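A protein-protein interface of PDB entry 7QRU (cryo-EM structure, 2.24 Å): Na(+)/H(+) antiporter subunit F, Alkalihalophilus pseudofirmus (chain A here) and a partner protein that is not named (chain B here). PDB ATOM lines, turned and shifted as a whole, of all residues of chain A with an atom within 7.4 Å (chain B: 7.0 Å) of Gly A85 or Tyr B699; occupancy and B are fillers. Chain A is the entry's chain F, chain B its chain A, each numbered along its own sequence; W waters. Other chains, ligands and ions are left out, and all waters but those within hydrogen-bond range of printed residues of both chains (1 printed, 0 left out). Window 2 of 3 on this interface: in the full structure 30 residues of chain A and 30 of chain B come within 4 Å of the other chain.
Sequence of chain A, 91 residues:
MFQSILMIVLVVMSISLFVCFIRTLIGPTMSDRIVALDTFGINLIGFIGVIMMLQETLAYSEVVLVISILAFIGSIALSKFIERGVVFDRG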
ATOM      1  N   SER A  79     -20.201  17.810   7.615  1.00  0.00           N
ATOM      2  CA  SER A  79     -18.976  18.407   8.109  1.00  0.00           C
ATOM      3  C   SER A  79     -17.843  18.299   7.115  1.00  0.00           C
ATOM      4  O   SER A  79     -17.034  19.197   7.005  1.00  0.00           O
ATOM      5  CB  SER A  79     -18.524  17.662   9.374  1.00  0.00           C
ATOM      6  OG  SER A  79     -19.254  18.227  10.422  1.00  0.00           O
ATOM      7  N   LYS A  80     -17.719  17.142   6.471  1.00  0.00           N
ATOM      8  CA  LYS A  80     -16.675  16.937   5.501  1.00  0.00           C
ATOM      9  C   LYS A  80     -16.947  17.736   4.222  1.00  0.00           C
ATOM     10  O   LYS A  80     -16.059  18.321   3.653  1.00  0.00           O
ATOM     11  CB  LYS A  80     -16.583  15.471   5.102  1.00  0.00           C
ATOM     12  CG  LYS A  80     -16.206  14.507   6.173  1.00  0.00           C
ATOM     13  CD  LYS A  80     -15.995  13.107   5.612  1.00  0.00           C
ATOM     14  CE  LYS A  80     -14.983  13.098   4.483  1.00  0.00           C
ATOM     15  NZ  LYS A  80     -14.637  11.673   4.227  1.00  0.00           N
ATOM     16  N   PHE A  81     -18.216  17.779   3.797  1.00  0.00           N
ATOM     17  CA  PHE A  81     -18.558  18.566   2.638  1.00  0.00           C
ATOM     18  C   PHE A  81     -18.084  19.991   2.847  1.00  0.00           C
ATOM     19  O   PHE A  81     -17.575  20.609   1.917  1.00  0.00           O
ATOM     20  CB  PHE A  81     -20.074  18.483   2.339  1.00  0.00           C
ATOM     21  CG  PHE A  81     -20.374  19.006   0.970  1.00  0.00           C
ATOM     22  CD1 PHE A  81     -19.891  18.351  -0.196  1.00  0.00           C
ATOM     23  CD2 PHE A  81     -20.886  20.297   0.879  1.00  0.00           C
ATOM     24  CE1 PHE A  81     -20.118  18.953  -1.426  1.00  0.00           C
ATOM     25  CE2 PHE A  81     -21.008  20.912  -0.363  1.00  0.00           C
ATOM     26  CZ  PHE A  81     -20.653  20.226  -1.508  1.00  0.00           C
ATOM     27  N   ILE A  82     -18.481  20.595   3.976  1.00  0.00           N
ATOM     28  CA  ILE A  82     -18.173  21.977   4.273  1.00  0.00           C
ATOM     29  C   ILE A  82     -16.653  22.192   4.227  1.00  0.00           C
ATOM     30  O   ILE A  82     -16.219  23.197   3.688  1.00  0.00           O
ATOM     31  CB  ILE A  82     -18.783  22.359   5.614  1.00  0.00           C
ATOM     32  CG1 ILE A  82     -20.266  22.579   5.428  1.00  0.00           C
ATOM     33  CG2 ILE A  82     -18.143  23.545   6.320  1.00  0.00           C
ATOM     34  CD1 ILE A  82     -20.901  22.616   6.938  1.00  0.00           C
ATOM     35  N   GLU A  83     -15.876  21.284   4.772  1.00  0.00           N
ATOM     36  CA  GLU A  83     -14.441  21.465   4.892  1.00  0.00           C
ATOM     37  C   GLU A  83     -13.716  21.157   3.565  1.00  0.00           C
ATOM     38  O   GLU A  83     -12.755  21.812   3.212  1.00  0.00           O
ATOM     39  CB  GLU A  83     -13.958  20.635   6.091  1.00  0.00           C
ATOM     40  CG  GLU A  83     -12.535  20.187   6.019  1.00  0.00           C
ATOM     41  CD  GLU A  83     -12.127  18.972   6.849  1.00  0.00           C
ATOM     42  OE1 GLU A  83     -12.896  18.525   7.734  1.00  0.00           O
ATOM     43  OE2 GLU A  83     -11.016  18.447   6.566  1.00  0.00           O
ATOM     44  N   ARG A  84     -14.095  20.140   2.843  1.00  0.00           N
ATOM     45  CA  ARG A  84     -13.342  19.651   1.695  1.00  0.00           C
ATOM     46  C   ARG A  84     -14.134  19.732   0.372  1.00  0.00           C
ATOM     47  O   ARG A  84     -13.498  19.799  -0.686  1.00  0.00           O
ATOM     48  CB  ARG A  84     -12.963  18.185   1.929  1.00  0.00           C
ATOM     49  CG  ARG A  84     -11.616  18.039   2.583  1.00  0.00           C
ATOM     50  CD  ARG A  84     -11.364  16.609   3.040  1.00  0.00           C
ATOM     51  NE  ARG A  84     -11.914  16.484   4.373  1.00  0.00           N
ATOM     52  CZ  ARG A  84     -11.893  15.379   5.101  1.00  0.00           C
ATOM     53  NH1 ARG A  84     -11.241  14.315   4.662  1.00  0.00           N
ATOM     54  NH2 ARG A  84     -12.668  15.295   6.176  1.00  0.00           N
ATOM     55  N   GLY A  85     -15.462  19.721   0.424  1.00  0.00           N
ATOM     56  CA  GLY A  85     -16.251  19.713  -0.762  1.00  0.00           C
ATOM     57  C   GLY A  85     -16.375  18.327  -1.367  1.00  0.00           C
ATOM     58  O   GLY A  85     -16.994  18.243  -2.409  1.00  0.00           O
ATOM     59  N   VAL A  86     -15.880  17.280  -0.687  1.00  0.00           N
ATOM     60  CA  VAL A  86     -16.115  15.901  -1.115  1.00  0.00           C
ATOM     61  C   VAL A  86     -16.677  15.127   0.076  1.00  0.00           C
ATOM     62  O   VAL A  86     -16.078  15.109   1.125  1.00  0.00           O
ATOM     63  CB  VAL A  86     -14.834  15.230  -1.648  1.00  0.00           C
ATOM     64  CG1 VAL A  86     -14.531  15.610  -3.075  1.00  0.00           C
ATOM     65  CG2 VAL A  86     -13.640  15.578  -0.809  1.00  0.00           C
ATOM     66  N   VAL A  87     -17.781  14.408  -0.022  1.00  0.00           N
ATOM     67  CA  VAL A  87     -18.171  13.430   1.008  1.00  0.00           C
ATOM     68  C   VAL A  87     -17.171  12.249   1.116  1.00  0.00           C
ATOM     69  O   VAL A  87     -16.847  11.837   2.209  1.00  0.00           O
ATOM     70  CB  VAL A  87     -19.592  12.900   0.730  1.00  0.00           C
ATOM     71  CG1 VAL A  87     -20.203  12.104   1.845  1.00  0.00           C
ATOM     72  CG2 VAL A  87     -20.492  14.120   0.578  1.00  0.00           C
ATOM     73  N   PHE A  88     -16.652  11.701   0.015  1.00  0.00           N
ATOM     74  CA  PHE A  88     -15.864  10.486   0.090  1.00  0.00           C
ATOM     75  C   PHE A  88     -14.464  10.742  -0.417  1.00  0.00           C
ATOM     76  O   PHE A  88     -14.335  11.274  -1.517  1.00  0.00           O
ATOM     77  CB  PHE A  88     -16.460   9.342  -0.767  1.00  0.00           C
ATOM     78  CG  PHE A  88     -17.834   8.872  -0.368  1.00  0.00           C
ATOM     79  CD1 PHE A  88     -18.131   8.244   0.850  1.00  0.00           C
ATOM     80  CD2 PHE A  88     -18.887   9.265  -1.099  1.00  0.00           C
ATOM     81  CE1 PHE A  88     -19.406   7.833   1.193  1.00  0.00           C
ATOM     82  CE2 PHE A  88     -20.172   8.841  -0.761  1.00  0.00           C
ATOM     83  CZ  PHE A  88     -20.434   8.128   0.385  1.00  0.00           C
ATOM     84  N   GLY A  91     -11.599   9.549  -4.420  1.00  0.00           N
ATOM     85  CA  GLY A  91     -12.333   9.103  -5.614  1.00  0.00           C
ATOM     86  C   GLY A  91     -12.300  10.067  -6.799  1.00  0.00           C
ATOM     87  O   GLY A  91     -11.903  11.230  -6.557  1.00  0.00           O
ATOM     88  OXT GLY A  91     -12.690   9.627  -7.928  1.00  0.00           O
ATOM     89  N   ARG B 653     -26.934  26.450  -1.249  1.00  0.00           N
ATOM     90  CA  ARG B 653     -27.420  25.101  -1.386  1.00  0.00           C
ATOM     91  C   ARG B 653     -27.219  24.324  -0.107  1.00  0.00           C
ATOM     92  O   ARG B 653     -28.003  23.442   0.096  1.00  0.00           O
ATOM     93  CB  ARG B 653     -26.769  24.324  -2.523  1.00  0.00           C
ATOM     94  CG  ARG B 653     -25.317  24.018  -2.280  1.00  0.00           C
ATOM     95  CD  ARG B 653     -24.717  23.837  -3.647  1.00  0.00           C
ATOM     96  NE  ARG B 653     -23.289  23.689  -3.502  1.00  0.00           N
ATOM     97  CZ  ARG B 653     -22.531  23.154  -4.429  1.00  0.00           C
ATOM     98  NH1 ARG B 653     -23.091  22.787  -5.584  1.00  0.00           N
ATOM     99  NH2 ARG B 653     -21.230  23.032  -4.209  1.00  0.00           N
ATOM    100  N   LEU B 694     -27.444  14.265  -2.599  1.00  0.00           N
ATOM    101  CA  LEU B 694     -27.434  15.710  -2.884  1.00  0.00           C
ATOM    102  C   LEU B 694     -26.034  16.269  -2.722  1.00  0.00           C
ATOM    103  O   LEU B 694     -25.557  16.915  -3.636  1.00  0.00           O
ATOM    104  CB  LEU B 694     -28.409  16.473  -2.016  1.00  0.00           C
ATOM    105  CG  LEU B 694     -29.822  16.329  -2.561  1.00  0.00           C
ATOM    106  CD1 LEU B 694     -30.812  16.533  -1.463  1.00  0.00           C
ATOM    107  CD2 LEU B 694     -30.048  17.358  -3.639  1.00  0.00           C
ATOM    108  N   MET B 695     -25.294  15.816  -1.745  1.00  0.00           N
ATOM    109  CA  MET B 695     -23.925  16.276  -1.636  1.00  0.00           C
ATOM    110  C   MET B 695     -22.980  15.675  -2.671  1.00  0.00           C
ATOM    111  O   MET B 695     -22.030  16.325  -3.038  1.00  0.00           O
ATOM    112  CB  MET B 695     -23.414  15.987  -0.216  1.00  0.00           C
ATOM    113  CG  MET B 695     -24.029  17.121   0.724  1.00  0.00           C
ATOM    114  SD  MET B 695     -23.318  16.714   2.240  1.00  0.00           S
ATOM    115  CE  MET B 695     -24.193  15.212   2.634  1.00  0.00           C
ATOM    116  N   LEU B 696     -23.147  14.437  -3.078  1.00  0.00           N
ATOM    117  CA  LEU B 696     -22.392  13.877  -4.182  1.00  0.00           C
ATOM    118  C   LEU B 696     -22.743  14.619  -5.474  1.00  0.00           C
ATOM    119  O   LEU B 696     -21.899  14.910  -6.266  1.00  0.00           O
ATOM    120  CB  LEU B 696     -22.750  12.424  -4.293  1.00  0.00           C
ATOM    121  CG  LEU B 696     -22.091  11.600  -3.224  1.00  0.00           C
ATOM    122  CD1 LEU B 696     -22.486  10.159  -3.403  1.00  0.00           C
ATOM    123  CD2 LEU B 696     -20.614  11.785  -3.326  1.00  0.00           C
ATOM    124  N   ALA B 697     -23.967  15.024  -5.644  1.00  0.00           N
ATOM    125  CA  ALA B 697     -24.309  15.828  -6.791  1.00  0.00           C
ATOM    126  C   ALA B 697     -23.759  17.247  -6.665  1.00  0.00           C
ATOM    127  O   ALA B 697     -23.610  17.867  -7.698  1.00  0.00           O
ATOM    128  CB  ALA B 697     -25.817  15.845  -6.978  1.00  0.00           C
ATOM    129  N   PHE B 698     -23.522  17.788  -5.453  1.00  0.00           N
ATOM    130  CA  PHE B 698     -23.117  19.199  -5.281  1.00  0.00           C
ATOM    131  C   PHE B 698     -21.667  19.395  -5.667  1.00  0.00           C
ATOM    132  O   PHE B 698     -21.212  20.516  -5.804  1.00  0.00           O
ATOM    133  CB  PHE B 698     -23.192  19.749  -3.835  1.00  0.00           C
ATOM    134  CG  PHE B 698     -24.612  20.080  -3.447  1.00  0.00           C
ATOM    135  CD1 PHE B 698     -25.664  19.904  -4.361  1.00  0.00           C
ATOM    136  CD2 PHE B 698     -24.913  20.395  -2.139  1.00  0.00           C
ATOM    137  CE1 PHE B 698     -26.974  20.163  -3.990  1.00  0.00           C
ATOM    138  CE2 PHE B 698     -26.224  20.679  -1.793  1.00  0.00           C
ATOM    139  CZ  PHE B 698     -27.248  20.559  -2.715  1.00  0.00           C
ATOM    140  N   TYR B 699     -20.920  18.275  -5.759  1.00  0.00           N
ATOM    141  CA  TYR B 699     -19.576  18.378  -6.268  1.00  0.00           C
ATOM    142  C   TYR B 699     -19.580  18.763  -7.773  1.00  0.00           C
ATOM    143  O   TYR B 699     -18.575  19.226  -8.309  1.00  0.00           O
ATOM    144  CB  TYR B 699     -18.842  17.090  -5.929  1.00  0.00           C
ATOM    145  CG  TYR B 699     -17.484  16.985  -6.598  1.00  0.00           C
ATOM    146  CD1 TYR B 699     -17.258  16.282  -7.788  1.00  0.00           C
ATOM    147  CD2 TYR B 699     -16.407  17.610  -6.017  1.00  0.00           C
ATOM    148  CE1 TYR B 699     -16.005  16.237  -8.383  1.00  0.00           C
ATOM    149  CE2 TYR B 699     -15.148  17.551  -6.590  1.00  0.00           C
ATOM    150  CZ  TYR B 699     -14.943  16.875  -7.779  1.00  0.00           C
ATOM    151  OH  TYR B 699     -13.712  16.801  -8.380  1.00  0.00           O
ATOM    152  N   HIS B 700     -20.682  18.488  -8.470  1.00  0.00           N
ATOM    153  CA  HIS B 700     -20.778  18.619  -9.910  1.00  0.00           C
ATOM    154  C   HIS B 700     -21.565  19.868 -10.245  1.00  0.00           C
ATOM    155  O   HIS B 700     -21.104  20.666 -11.044  1.00  0.00           O
ATOM    156  CB  HIS B 700     -21.439  17.356 -10.444  1.00  0.00           C
ATOM    157  CG  HIS B 700     -20.504  16.197 -10.447  1.00  0.00           C
ATOM    158  ND1 HIS B 700     -19.428  16.101 -11.346  1.00  0.00           N
ATOM    159  CD2 HIS B 700     -20.569  15.046  -9.736  1.00  0.00           C
ATOM    160  CE1 HIS B 700     -18.847  14.925 -11.115  1.00  0.00           C
ATOM    161  NE2 HIS B 700     -19.537  14.231 -10.142  1.00  0.00           N
ATOM    162  N   LEU B 701     -22.580  20.162  -9.415  1.00  0.00           N
ATOM    163  CA  LEU B 701     -23.471  21.307  -9.626  1.00  0.00           C
ATOM    164  C   LEU B 701     -22.822  22.583  -9.130  1.00  0.00           C
ATOM    165  O   LEU B 701     -21.814  22.535  -8.452  1.00  0.00           O
ATOM    166  CB  LEU B 701     -24.804  21.070  -8.922  1.00  0.00           C
ATOM    167  CG  LEU B 701     -25.600  20.002  -9.647  1.00  0.00           C
ATOM    168  CD1 LEU B 701     -26.575  19.370  -8.698  1.00  0.00           C
ATOM    169  CD2 LEU B 701     -26.216  20.609 -10.904  1.00  0.00           C
ATOM    170  N   PRO B 702     -23.311  23.735  -9.618  1.00  0.00           N
ATOM    171  CA  PRO B 702     -22.892  25.029  -9.090  1.00  0.00           C
ATOM    172  C   PRO B 702     -23.606  25.403  -7.780  1.00  0.00           C
ATOM    173  O   PRO B 702     -24.537  24.714  -7.409  1.00  0.00           O
ATOM    174  CB  PRO B 702     -23.292  25.911 -10.265  1.00  0.00           C
ATOM    175  CG  PRO B 702     -24.578  25.303 -10.742  1.00  0.00           C
ATOM    176  CD  PRO B 702     -24.342  23.832 -10.671  1.00  0.00           C
HETATM  177  O   HOH W   1     -18.990  15.335  -2.959  1.00  0.00           O
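NH1 of Arg B653 lies within hydrogen-bond range of O of Phe B698, at 3.0 Å.
The backbone carbonyl oxygen (O) of Leu B701 is in hydrogen-bond range of the guanidinium group (NH1) of Arg B653, 3.1 Å away.
The backbone carbonyl oxygen (O) of Pro B702 lies within hydrogen-bond range of the guanidinium group (NH1) of Arg B653 (3.0 Å).
The side-chain amino group (NZ) of Lys A80 sits at hydrogen-bond distance from the backbone carbonyl oxygen (O) of Val A87, at 3.0 Å.
Water W1 lies within hydrogen-bond range of the backbone carbonyl oxygen of Met B695 (3.2 Å) and the backbone NH of Val A87 (3.3 Å).
Gly A85 touches just one residue of chain B: Tyr B699.
Of the printed residues of chain A, Arg B653 touches Phe A81.
Of the printed residues of chain A, Met B695 touches Phe A81 (3.6 Å) and Val A87 (3.6 Å).
Printed residues of chain A within 4 Å of Phe B698: Phe A81.
Tyr B699 touches just one residue of chain A: Gly A85 (3.7 Å).
The nearest residue of chain B that does not touch Gly A85 is Met B695 (5.4 Å).
The nearest residue of chain A that does not touch Tyr B699 is Val A86 (4.02 Å).
The nearest printed residue of chain B that does not touch Phe A88 is Met B695 (7.6 Å).
CZ of Phe A81 touches NH2 of Arg B653, at 3.9 Å.
Phe A81 touches Met B695.
Phe A81 touches Phe B698.
Gly A85 touches Tyr B699 (O to CD2, 3.7 Å).
Val A87 touches Met B695.
Leu B696 touches Phe A88.
Of the 11 printed residues of chain A, 4 touch a printed residue of chain B.
Hydrophobic or aromatic side chains of chain A within 4 Å of the printed part of chain B: Phe A81, Val A87 and Phe A88.
Among the printed residues, no Asp or Glu carboxylate lies within 4 Å of a Lys or Arg side-chain nitrogen of the other chain.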
